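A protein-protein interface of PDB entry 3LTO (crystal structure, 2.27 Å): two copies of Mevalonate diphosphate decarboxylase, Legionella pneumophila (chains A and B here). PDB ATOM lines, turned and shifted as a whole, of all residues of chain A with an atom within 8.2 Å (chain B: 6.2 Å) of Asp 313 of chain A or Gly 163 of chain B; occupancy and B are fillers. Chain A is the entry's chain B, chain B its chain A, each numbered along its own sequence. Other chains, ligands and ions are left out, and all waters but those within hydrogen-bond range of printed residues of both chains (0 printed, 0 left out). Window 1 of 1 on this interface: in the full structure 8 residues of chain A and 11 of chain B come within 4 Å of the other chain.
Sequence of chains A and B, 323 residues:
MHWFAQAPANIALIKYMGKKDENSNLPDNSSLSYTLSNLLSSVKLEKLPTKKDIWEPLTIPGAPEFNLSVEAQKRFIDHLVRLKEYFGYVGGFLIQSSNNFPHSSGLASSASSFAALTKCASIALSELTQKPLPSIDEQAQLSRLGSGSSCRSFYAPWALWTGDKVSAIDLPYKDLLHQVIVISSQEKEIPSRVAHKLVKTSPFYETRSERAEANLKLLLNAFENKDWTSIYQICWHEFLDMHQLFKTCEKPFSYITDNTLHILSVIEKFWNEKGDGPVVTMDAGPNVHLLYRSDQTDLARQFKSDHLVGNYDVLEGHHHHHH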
ATOM      1  N   SER A 105      -6.199  34.437   9.683  1.00  0.00           N
ATOM      2  CA  SER A 105      -6.726  33.162  10.148  1.00  0.00           C
ATOM      3  C   SER A 105      -8.155  33.056   9.625  1.00  0.00           C
ATOM      4  O   SER A 105      -9.040  32.562  10.315  1.00  0.00           O
ATOM      5  CB  SER A 105      -6.727  33.127  11.679  1.00  0.00           C
ATOM      6  OG  SER A 105      -5.508  33.634  12.198  1.00  0.00           O
ATOM      7  N   GLN A 179     -18.387  29.883  16.563  1.00  0.00           N
ATOM      8  CA  GLN A 179     -16.976  29.553  16.778  1.00  0.00           C
ATOM      9  C   GLN A 179     -16.364  29.215  15.428  1.00  0.00           C
ATOM     10  O   GLN A 179     -17.027  28.645  14.560  1.00  0.00           O
ATOM     11  CB  GLN A 179     -16.810  28.348  17.717  1.00  0.00           C
ATOM     12  CG  GLN A 179     -17.454  28.490  19.091  1.00  0.00           C
ATOM     13  CD  GLN A 179     -17.127  27.315  20.003  1.00  0.00           C
ATOM     14  OE1 GLN A 179     -17.128  26.165  19.572  1.00  0.00           O
ATOM     15  NE2 GLN A 179     -16.852  27.604  21.271  1.00  0.00           N
ATOM     16  N   VAL A 180     -15.097  29.563  15.259  1.00  0.00           N
ATOM     17  CA  VAL A 180     -14.395  29.314  14.016  1.00  0.00           C
ATOM     18  C   VAL A 180     -13.214  28.396  14.253  1.00  0.00           C
ATOM     19  O   VAL A 180     -12.376  28.685  15.096  1.00  0.00           O
ATOM     20  CB  VAL A 180     -13.844  30.634  13.410  1.00  0.00           C
ATOM     21  CG1 VAL A 180     -13.318  30.385  12.004  1.00  0.00           C
ATOM     22  CG2 VAL A 180     -14.926  31.701  13.406  1.00  0.00           C
ATOM     23  N   ILE A 181     -13.160  27.286  13.521  1.00  0.00           N
ATOM     24  CA  ILE A 181     -12.032  26.368  13.625  1.00  0.00           C
ATOM     25  C   ILE A 181     -11.033  26.937  12.622  1.00  0.00           C
ATOM     26  O   ILE A 181     -11.332  27.009  11.425  1.00  0.00           O
ATOM     27  CB  ILE A 181     -12.374  24.953  13.151  1.00  0.00           C
ATOM     28  CG1 ILE A 181     -13.616  24.427  13.867  1.00  0.00           C
ATOM     29  CG2 ILE A 181     -11.180  24.044  13.401  1.00  0.00           C
ATOM     30  CD1 ILE A 181     -13.403  24.134  15.292  1.00  0.00           C
ATOM     31  N   VAL A 182      -9.857  27.329  13.097  1.00  0.00           N
ATOM     32  CA  VAL A 182      -8.851  27.915  12.220  1.00  0.00           C
ATOM     33  C   VAL A 182      -7.892  26.945  11.550  1.00  0.00           C
ATOM     34  O   VAL A 182      -7.069  26.309  12.205  1.00  0.00           O
ATOM     35  CB  VAL A 182      -8.004  28.962  12.968  1.00  0.00           C
ATOM     36  CG1 VAL A 182      -6.905  29.492  12.055  1.00  0.00           C
ATOM     37  CG2 VAL A 182      -8.891  30.096  13.436  1.00  0.00           C
ATOM     38  N   ILE A 183      -8.007  26.849  10.230  1.00  0.00           N
ATOM     39  CA  ILE A 183      -7.136  26.003   9.424  1.00  0.00           C
ATOM     40  C   ILE A 183      -6.306  26.990   8.602  1.00  0.00           C
ATOM     41  O   ILE A 183      -6.841  27.662   7.727  1.00  0.00           O
ATOM     42  CB  ILE A 183      -7.936  25.120   8.440  1.00  0.00           C
ATOM     43  CG1 ILE A 183      -8.980  24.283   9.185  1.00  0.00           C
ATOM     44  CG2 ILE A 183      -6.982  24.231   7.663  1.00  0.00           C
ATOM     45  CD1 ILE A 183      -8.427  23.098   9.928  1.00  0.00           C
ATOM     46  N   SER A 184      -5.014  27.087   8.893  1.00  0.00           N
ATOM     47  CA  SER A 184      -4.124  28.004   8.180  1.00  0.00           C
ATOM     48  C   SER A 184      -4.109  27.789   6.667  1.00  0.00           C
ATOM     49  O   SER A 184      -4.098  26.652   6.191  1.00  0.00           O
ATOM     50  CB  SER A 184      -2.701  27.871   8.721  1.00  0.00           C
ATOM     51  OG  SER A 184      -1.796  28.644   7.949  1.00  0.00           O
ATOM     52  N   ASN A 287     -11.251  28.066   6.773  1.00  0.00           N
ATOM     53  CA  ASN A 287     -11.898  27.991   8.087  1.00  0.00           C
ATOM     54  C   ASN A 287     -13.208  27.201   8.136  1.00  0.00           C
ATOM     55  O   ASN A 287     -13.951  27.140   7.158  1.00  0.00           O
ATOM     56  CB  ASN A 287     -12.169  29.398   8.629  1.00  0.00           C
ATOM     57  CG  ASN A 287     -10.907  30.116   9.081  1.00  0.00           C
ATOM     58  OD1 ASN A 287     -10.961  31.288   9.462  1.00  0.00           O
ATOM     59  ND2 ASN A 287      -9.773  29.427   9.042  1.00  0.00           N
ATOM     60  N   VAL A 288     -13.494  26.618   9.295  1.00  0.00           N
ATOM     61  CA  VAL A 288     -14.725  25.858   9.480  1.00  0.00           C
ATOM     62  C   VAL A 288     -15.560  26.558  10.546  1.00  0.00           C
ATOM     63  O   VAL A 288     -15.101  26.791  11.661  1.00  0.00           O
ATOM     64  CB  VAL A 288     -14.429  24.404   9.918  1.00  0.00           C
ATOM     65  CG1 VAL A 288     -15.729  23.647  10.141  1.00  0.00           C
ATOM     66  CG2 VAL A 288     -13.570  23.710   8.858  1.00  0.00           C
ATOM     67  N   LYS A 304     -15.338  21.275  22.299  1.00  0.00           N
ATOM     68  CA  LYS A 304     -14.109  22.052  22.249  1.00  0.00           C
ATOM     69  C   LYS A 304     -13.005  21.403  23.071  1.00  0.00           C
ATOM     70  O   LYS A 304     -11.873  21.255  22.607  1.00  0.00           O
ATOM     71  CB  LYS A 304     -14.372  23.473  22.753  1.00  0.00           C
ATOM     72  CG  LYS A 304     -13.181  24.401  22.652  1.00  0.00           C
ATOM     73  CD  LYS A 304     -13.548  25.821  23.053  1.00  0.00           C
ATOM     74  CE  LYS A 304     -12.320  26.722  23.040  1.00  0.00           C
ATOM     75  NZ  LYS A 304     -12.653  28.141  23.372  1.00  0.00           N
ATOM     76  N   LEU A 308     -11.131  20.069  20.151  1.00  0.00           N
ATOM     77  CA  LEU A 308     -10.426  21.240  19.624  1.00  0.00           C
ATOM     78  C   LEU A 308      -9.166  21.609  20.395  1.00  0.00           C
ATOM     79  O   LEU A 308      -8.149  21.956  19.798  1.00  0.00           O
ATOM     80  CB  LEU A 308     -11.359  22.457  19.569  1.00  0.00           C
ATOM     81  CG  LEU A 308     -12.582  22.325  18.657  1.00  0.00           C
ATOM     82  CD1 LEU A 308     -13.347  23.637  18.624  1.00  0.00           C
ATOM     83  CD2 LEU A 308     -12.127  21.934  17.250  1.00  0.00           C
ATOM     84  N   VAL A 309      -9.238  21.541  21.717  1.00  0.00           N
ATOM     85  CA  VAL A 309      -8.094  21.883  22.550  1.00  0.00           C
ATOM     86  C   VAL A 309      -6.844  21.084  22.168  1.00  0.00           C
ATOM     87  O   VAL A 309      -6.875  19.851  22.094  1.00  0.00           O
ATOM     88  CB  VAL A 309      -8.411  21.638  24.031  1.00  0.00           C
ATOM     89  CG1 VAL A 309      -7.190  21.959  24.887  1.00  0.00           C
ATOM     90  CG2 VAL A 309      -9.598  22.497  24.452  1.00  0.00           C
ATOM     91  N   GLY A 310      -5.752  21.798  21.913  1.00  0.00           N
ATOM     92  CA  GLY A 310      -4.508  21.145  21.554  1.00  0.00           C
ATOM     93  C   GLY A 310      -4.380  20.696  20.106  1.00  0.00           C
ATOM     94  O   GLY A 310      -3.319  20.212  19.709  1.00  0.00           O
ATOM     95  N   ASN A 311      -5.442  20.859  19.318  1.00  0.00           N
ATOM     96  CA  ASN A 311      -5.423  20.457  17.913  1.00  0.00           C
ATOM     97  C   ASN A 311      -5.686  21.613  16.945  1.00  0.00           C
ATOM     98  O   ASN A 311      -5.052  21.701  15.895  1.00  0.00           O
ATOM     99  CB  ASN A 311      -6.463  19.360  17.665  1.00  0.00           C
ATOM    100  CG  ASN A 311      -6.253  18.145  18.549  1.00  0.00           C
ATOM    101  OD1 ASN A 311      -7.180  17.683  19.215  1.00  0.00           O
ATOM    102  ND2 ASN A 311      -5.037  17.616  18.550  1.00  0.00           N
ATOM    103  N   TYR A 312      -6.617  22.497  17.298  1.00  0.00           N
ATOM    104  CA  TYR A 312      -6.964  23.627  16.439  1.00  0.00           C
ATOM    105  C   TYR A 312      -7.197  24.912  17.226  1.00  0.00           C
ATOM    106  O   TYR A 312      -7.634  24.877  18.373  1.00  0.00           O
ATOM    107  CB  TYR A 312      -8.250  23.321  15.656  1.00  0.00           C
ATOM    108  CG  TYR A 312      -8.230  22.045  14.842  1.00  0.00           C
ATOM    109  CD1 TYR A 312      -7.656  22.012  13.574  1.00  0.00           C
ATOM    110  CD2 TYR A 312      -8.781  20.871  15.345  1.00  0.00           C
ATOM    111  CE1 TYR A 312      -7.632  20.835  12.824  1.00  0.00           C
ATOM    112  CE2 TYR A 312      -8.760  19.697  14.613  1.00  0.00           C
ATOM    113  CZ  TYR A 312      -8.185  19.682  13.350  1.00  0.00           C
ATOM    114  OH  TYR A 312      -8.156  18.513  12.618  1.00  0.00           O
ATOM    115  N   ASP A 313      -6.902  26.050  16.608  1.00  0.00           N
ATOM    116  CA  ASP A 313      -7.158  27.332  17.252  1.00  0.00           C
ATOM    117  C   ASP A 313      -8.639  27.613  17.041  1.00  0.00           C
ATOM    118  O   ASP A 313      -9.168  27.390  15.953  1.00  0.00           O
ATOM    119  CB  ASP A 313      -6.342  28.464  16.614  1.00  0.00           C
ATOM    120  CG  ASP A 313      -4.895  28.465  17.057  1.00  0.00           C
ATOM    121  OD1 ASP A 313      -4.649  28.359  18.280  1.00  0.00           O
ATOM    122  OD2 ASP A 313      -4.005  28.588  16.187  1.00  0.00           O
ATOM    123  N   VAL A 314      -9.306  28.097  18.079  1.00  0.00           N
ATOM    124  CA  VAL A 314     -10.725  28.410  17.974  1.00  0.00           C
ATOM    125  C   VAL A 314     -10.933  29.892  18.255  1.00  0.00           C
ATOM    126  O   VAL A 314     -10.376  30.437  19.209  1.00  0.00           O
ATOM    127  CB  VAL A 314     -11.553  27.582  18.973  1.00  0.00           C
ATOM    128  CG1 VAL A 314     -13.031  27.715  18.660  1.00  0.00           C
ATOM    129  CG2 VAL A 314     -11.124  26.127  18.911  1.00  0.00           C
ATOM    130  N   LEU A 315     -11.728  30.544  17.415  1.00  0.00           N
ATOM    131  CA  LEU A 315     -12.006  31.962  17.575  1.00  0.00           C
ATOM    132  C   LEU A 315     -13.385  32.112  18.198  1.00  0.00           C
ATOM    133  O   LEU A 315     -14.307  31.448  17.679  1.00  0.00           O
ATOM    134  CB  LEU A 315     -11.988  32.646  16.212  1.00  0.00           C
ATOM    135  CG  LEU A 315     -10.866  32.150  15.302  1.00  0.00           C
ATOM    136  CD1 LEU A 315     -11.025  32.749  13.907  1.00  0.00           C
ATOM    137  CD2 LEU A 315      -9.518  32.513  15.915  1.00  0.00           C
ATOM    138  N   LEU B  26       3.978  29.253  12.147  1.00  0.00           N
ATOM    139  CA  LEU B  26       3.154  28.584  13.151  1.00  0.00           C
ATOM    140  C   LEU B  26       3.781  27.216  13.449  1.00  0.00           C
ATOM    141  O   LEU B  26       4.345  26.584  12.560  1.00  0.00           O
ATOM    142  CB  LEU B  26       1.734  28.393  12.614  1.00  0.00           C
ATOM    143  CG  LEU B  26       0.947  29.669  12.302  1.00  0.00           C
ATOM    144  CD1 LEU B  26      -0.248  29.339  11.414  1.00  0.00           C
ATOM    145  CD2 LEU B  26       0.498  30.319  13.601  1.00  0.00           C
ATOM    146  N   PRO B  27       3.692  26.748  14.705  1.00  0.00           N
ATOM    147  CA  PRO B  27       4.271  25.445  15.061  1.00  0.00           C
ATOM    148  C   PRO B  27       3.543  24.295  14.377  1.00  0.00           C
ATOM    149  O   PRO B  27       2.323  24.331  14.231  1.00  0.00           O
ATOM    150  CB  PRO B  27       4.122  25.403  16.581  1.00  0.00           C
ATOM    151  CG  PRO B  27       2.853  26.206  16.814  1.00  0.00           C
ATOM    152  CD  PRO B  27       3.030  27.374  15.867  1.00  0.00           C
ATOM    153  N   ASN B  29       3.167  21.432  15.551  1.00  0.00           N
ATOM    154  CA  ASN B  29       2.354  20.772  16.550  1.00  0.00           C
ATOM    155  C   ASN B  29       2.340  21.595  17.815  1.00  0.00           C
ATOM    156  O   ASN B  29       3.200  22.443  18.029  1.00  0.00           O
ATOM    157  CB  ASN B  29       2.825  19.331  16.831  1.00  0.00           C
ATOM    158  CG  ASN B  29       4.259  19.252  17.317  1.00  0.00           C
ATOM    159  OD1 ASN B  29       5.171  18.946  16.543  1.00  0.00           O
ATOM    160  ND2 ASN B  29       4.467  19.520  18.604  1.00  0.00           N
ATOM    161  N   SER B  30       1.328  21.366  18.635  1.00  0.00           N
ATOM    162  CA  SER B  30       1.204  22.083  19.882  1.00  0.00           C
ATOM    163  C   SER B  30       2.305  21.633  20.827  1.00  0.00           C
ATOM    164  O   SER B  30       2.989  20.627  20.585  1.00  0.00           O
ATOM    165  CB  SER B  30      -0.158  21.802  20.516  1.00  0.00           C
ATOM    166  OG  SER B  30      -1.205  22.247  19.676  1.00  0.00           O
ATOM    167  N   TRP B 161       0.563  25.799  23.968  1.00  0.00           N
ATOM    168  CA  TRP B 161       0.769  26.574  22.754  1.00  0.00           C
ATOM    169  C   TRP B 161       0.209  25.774  21.580  1.00  0.00           C
ATOM    170  O   TRP B 161       0.659  24.664  21.296  1.00  0.00           O
ATOM    171  CB  TRP B 161       2.274  26.841  22.592  1.00  0.00           C
ATOM    172  CG  TRP B 161       2.709  27.558  21.340  1.00  0.00           C
ATOM    173  CD1 TRP B 161       1.928  28.267  20.478  1.00  0.00           C
ATOM    174  CD2 TRP B 161       4.046  27.646  20.835  1.00  0.00           C
ATOM    175  NE1 TRP B 161       2.694  28.793  19.460  1.00  0.00           N
ATOM    176  CE2 TRP B 161       4.000  28.429  19.656  1.00  0.00           C
ATOM    177  CE3 TRP B 161       5.283  27.140  21.263  1.00  0.00           C
ATOM    178  CZ2 TRP B 161       5.144  28.717  18.897  1.00  0.00           C
ATOM    179  CZ3 TRP B 161       6.421  27.421  20.512  1.00  0.00           C
ATOM    180  CH2 TRP B 161       6.342  28.206  19.340  1.00  0.00           C
ATOM    181  N   THR B 162      -0.802  26.332  20.927  1.00  0.00           N
ATOM    182  CA  THR B 162      -1.430  25.695  19.778  1.00  0.00           C
ATOM    183  C   THR B 162      -1.619  26.767  18.725  1.00  0.00           C
ATOM    184  O   THR B 162      -2.213  27.802  19.002  1.00  0.00           O
ATOM    185  CB  THR B 162      -2.811  25.116  20.133  1.00  0.00           C
ATOM    186  OG1 THR B 162      -2.658  24.014  21.032  1.00  0.00           O
ATOM    187  CG2 THR B 162      -3.522  24.643  18.880  1.00  0.00           C
ATOM    188  N   GLY B 163      -1.120  26.525  17.519  1.00  0.00           N
ATOM    189  CA  GLY B 163      -1.255  27.517  16.470  1.00  0.00           C
ATOM    190  C   GLY B 163      -0.537  28.793  16.868  1.00  0.00           C
ATOM    191  O   GLY B 163       0.619  28.751  17.301  1.00  0.00           O
ATOM    192  N   ASP B 164      -1.207  29.935  16.737  1.00  0.00           N
ATOM    193  CA  ASP B 164      -0.570  31.194  17.107  1.00  0.00           C
ATOM    194  C   ASP B 164      -1.068  31.707  18.449  1.00  0.00           C
ATOM    195  O   ASP B 164      -0.917  32.890  18.762  1.00  0.00           O
ATOM    196  CB  ASP B 164      -0.778  32.266  16.025  1.00  0.00           C
ATOM    197  CG  ASP B 164      -2.237  32.612  15.810  1.00  0.00           C
ATOM    198  OD1 ASP B 164      -2.972  32.739  16.811  1.00  0.00           O
ATOM    199  OD2 ASP B 164      -2.646  32.774  14.641  1.00  0.00           O
ATOM    200  N   LYS B 165      -1.657  30.813  19.241  1.00  0.00           N
ATOM    201  CA  LYS B 165      -2.162  31.185  20.556  1.00  0.00           C
ATOM    202  C   LYS B 165      -1.494  30.390  21.672  1.00  0.00           C
ATOM    203  O   LYS B 165      -1.295  29.180  21.560  1.00  0.00           O
ATOM    204  CB  LYS B 165      -3.676  30.970  20.631  1.00  0.00           C
ATOM    205  CG  LYS B 165      -4.288  31.390  21.962  1.00  0.00           C
ATOM    206  CD  LYS B 165      -5.678  30.808  22.155  1.00  0.00           C
ATOM    207  CE  LYS B 165      -6.228  31.149  23.533  1.00  0.00           C
ATOM    208  NZ  LYS B 165      -7.527  30.468  23.786  1.00  0.00           N
ATOM    209  N   VAL B 166      -1.140  31.088  22.745  1.00  0.00           N
ATOM    210  CA  VAL B 166      -0.519  30.465  23.904  1.00  0.00           C
ATOM    211  C   VAL B 166      -1.329  30.887  25.118  1.00  0.00           C
ATOM    212  O   VAL B 166      -1.700  32.046  25.248  1.00  0.00           O
ATOM    213  CB  VAL B 166       0.938  30.934  24.103  1.00  0.00           C
ATOM    214  CG1 VAL B 166       1.547  30.223  25.304  1.00  0.00           C
ATOM    215  CG2 VAL B 166       1.747  30.663  22.855  1.00  0.00           C
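OD1 of Asp 313 of chain A lies close to O of Thr 162 of chain B. The backbone NH of Asp 164 of chain B lies within hydrogen-bond range of the side-chain carboxylate of Asp 313 of chain A. The side-chain hydroxyl (OG) of Ser 30 of chain B lies within hydrogen-bond range of the backbone carbonyl oxygen (O) of Gly 310 of chain A, at 2.9 Å.
O of Asp 313 of chain A is in hydrogen-bond range of N of Val 182 of chain A. OG1 of Thr 162 of chain B lies within hydrogen-bond range of OG of Ser 30 of chain B. OD1 of Asn 287 of chain A lies close to O of Ser 105 of chain A, 2.5 Å away. NE1 of Trp 161 of chain B sits at hydrogen-bond distance from O of Gly 163 of chain B (3.0 Å). OG of Ser 30 of chain B lies close to O of Trp 161 of chain B (3.5 Å).
Asp 164 of chain B touches Ser 105 of chain A (OD2 to OG, 3.9 Å). Ser 184 of chain A touches Leu 26 of chain B. Gly 310 of chain A touches Thr 162 of chain B. Asp 313 of chain A touches Gly 163 of chain B (OD2 to CA, 3.0 Å). Lys 165 of chain B touches Asp 313 of chain A.
Asp 313 of chain A touches four residues of chain B. Of the printed residues of chain A, Gly 163 of chain B touches Asp 313 (3.0 Å). Of the printed residues of chain B, Gly 310 of chain A touches Ser 30 (2.9 Å) and Thr 162 (3.5 Å). Of the printed residues of chain A, Lys 165 of chain B touches Asp 313 (3.6 Å). Of the printed residues of chain B, Ser 184 of chain A touches Leu 26 (3.9 Å). Of the printed residues of chain A, Thr 162 of chain B touches Gly 310 (3.5 Å) and Asp 313 (2.6 Å). Printed residues of chain A within 4 Å of Ser 30 of chain B: Gly 310 (2.9 Å). The nearest residue of chain B that does not touch Asp 313 of chain A is Leu 26 of chain B (5.5 Å). The nearest printed residue of chain A that does not touch Asp 164 of chain B is Val 182 of chain A (6.0 Å).
Of the 18 printed residues of chain A, 4 touch a printed residue of chain B. Hydrophobic or aromatic side chains of chain B within 4 Å of the printed part of chain A: Leu 26.
No position is printed for both chains. Of the 8 pairs that touch across the chains among the printed residues, none has its exchanged pair printed and touching as well.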
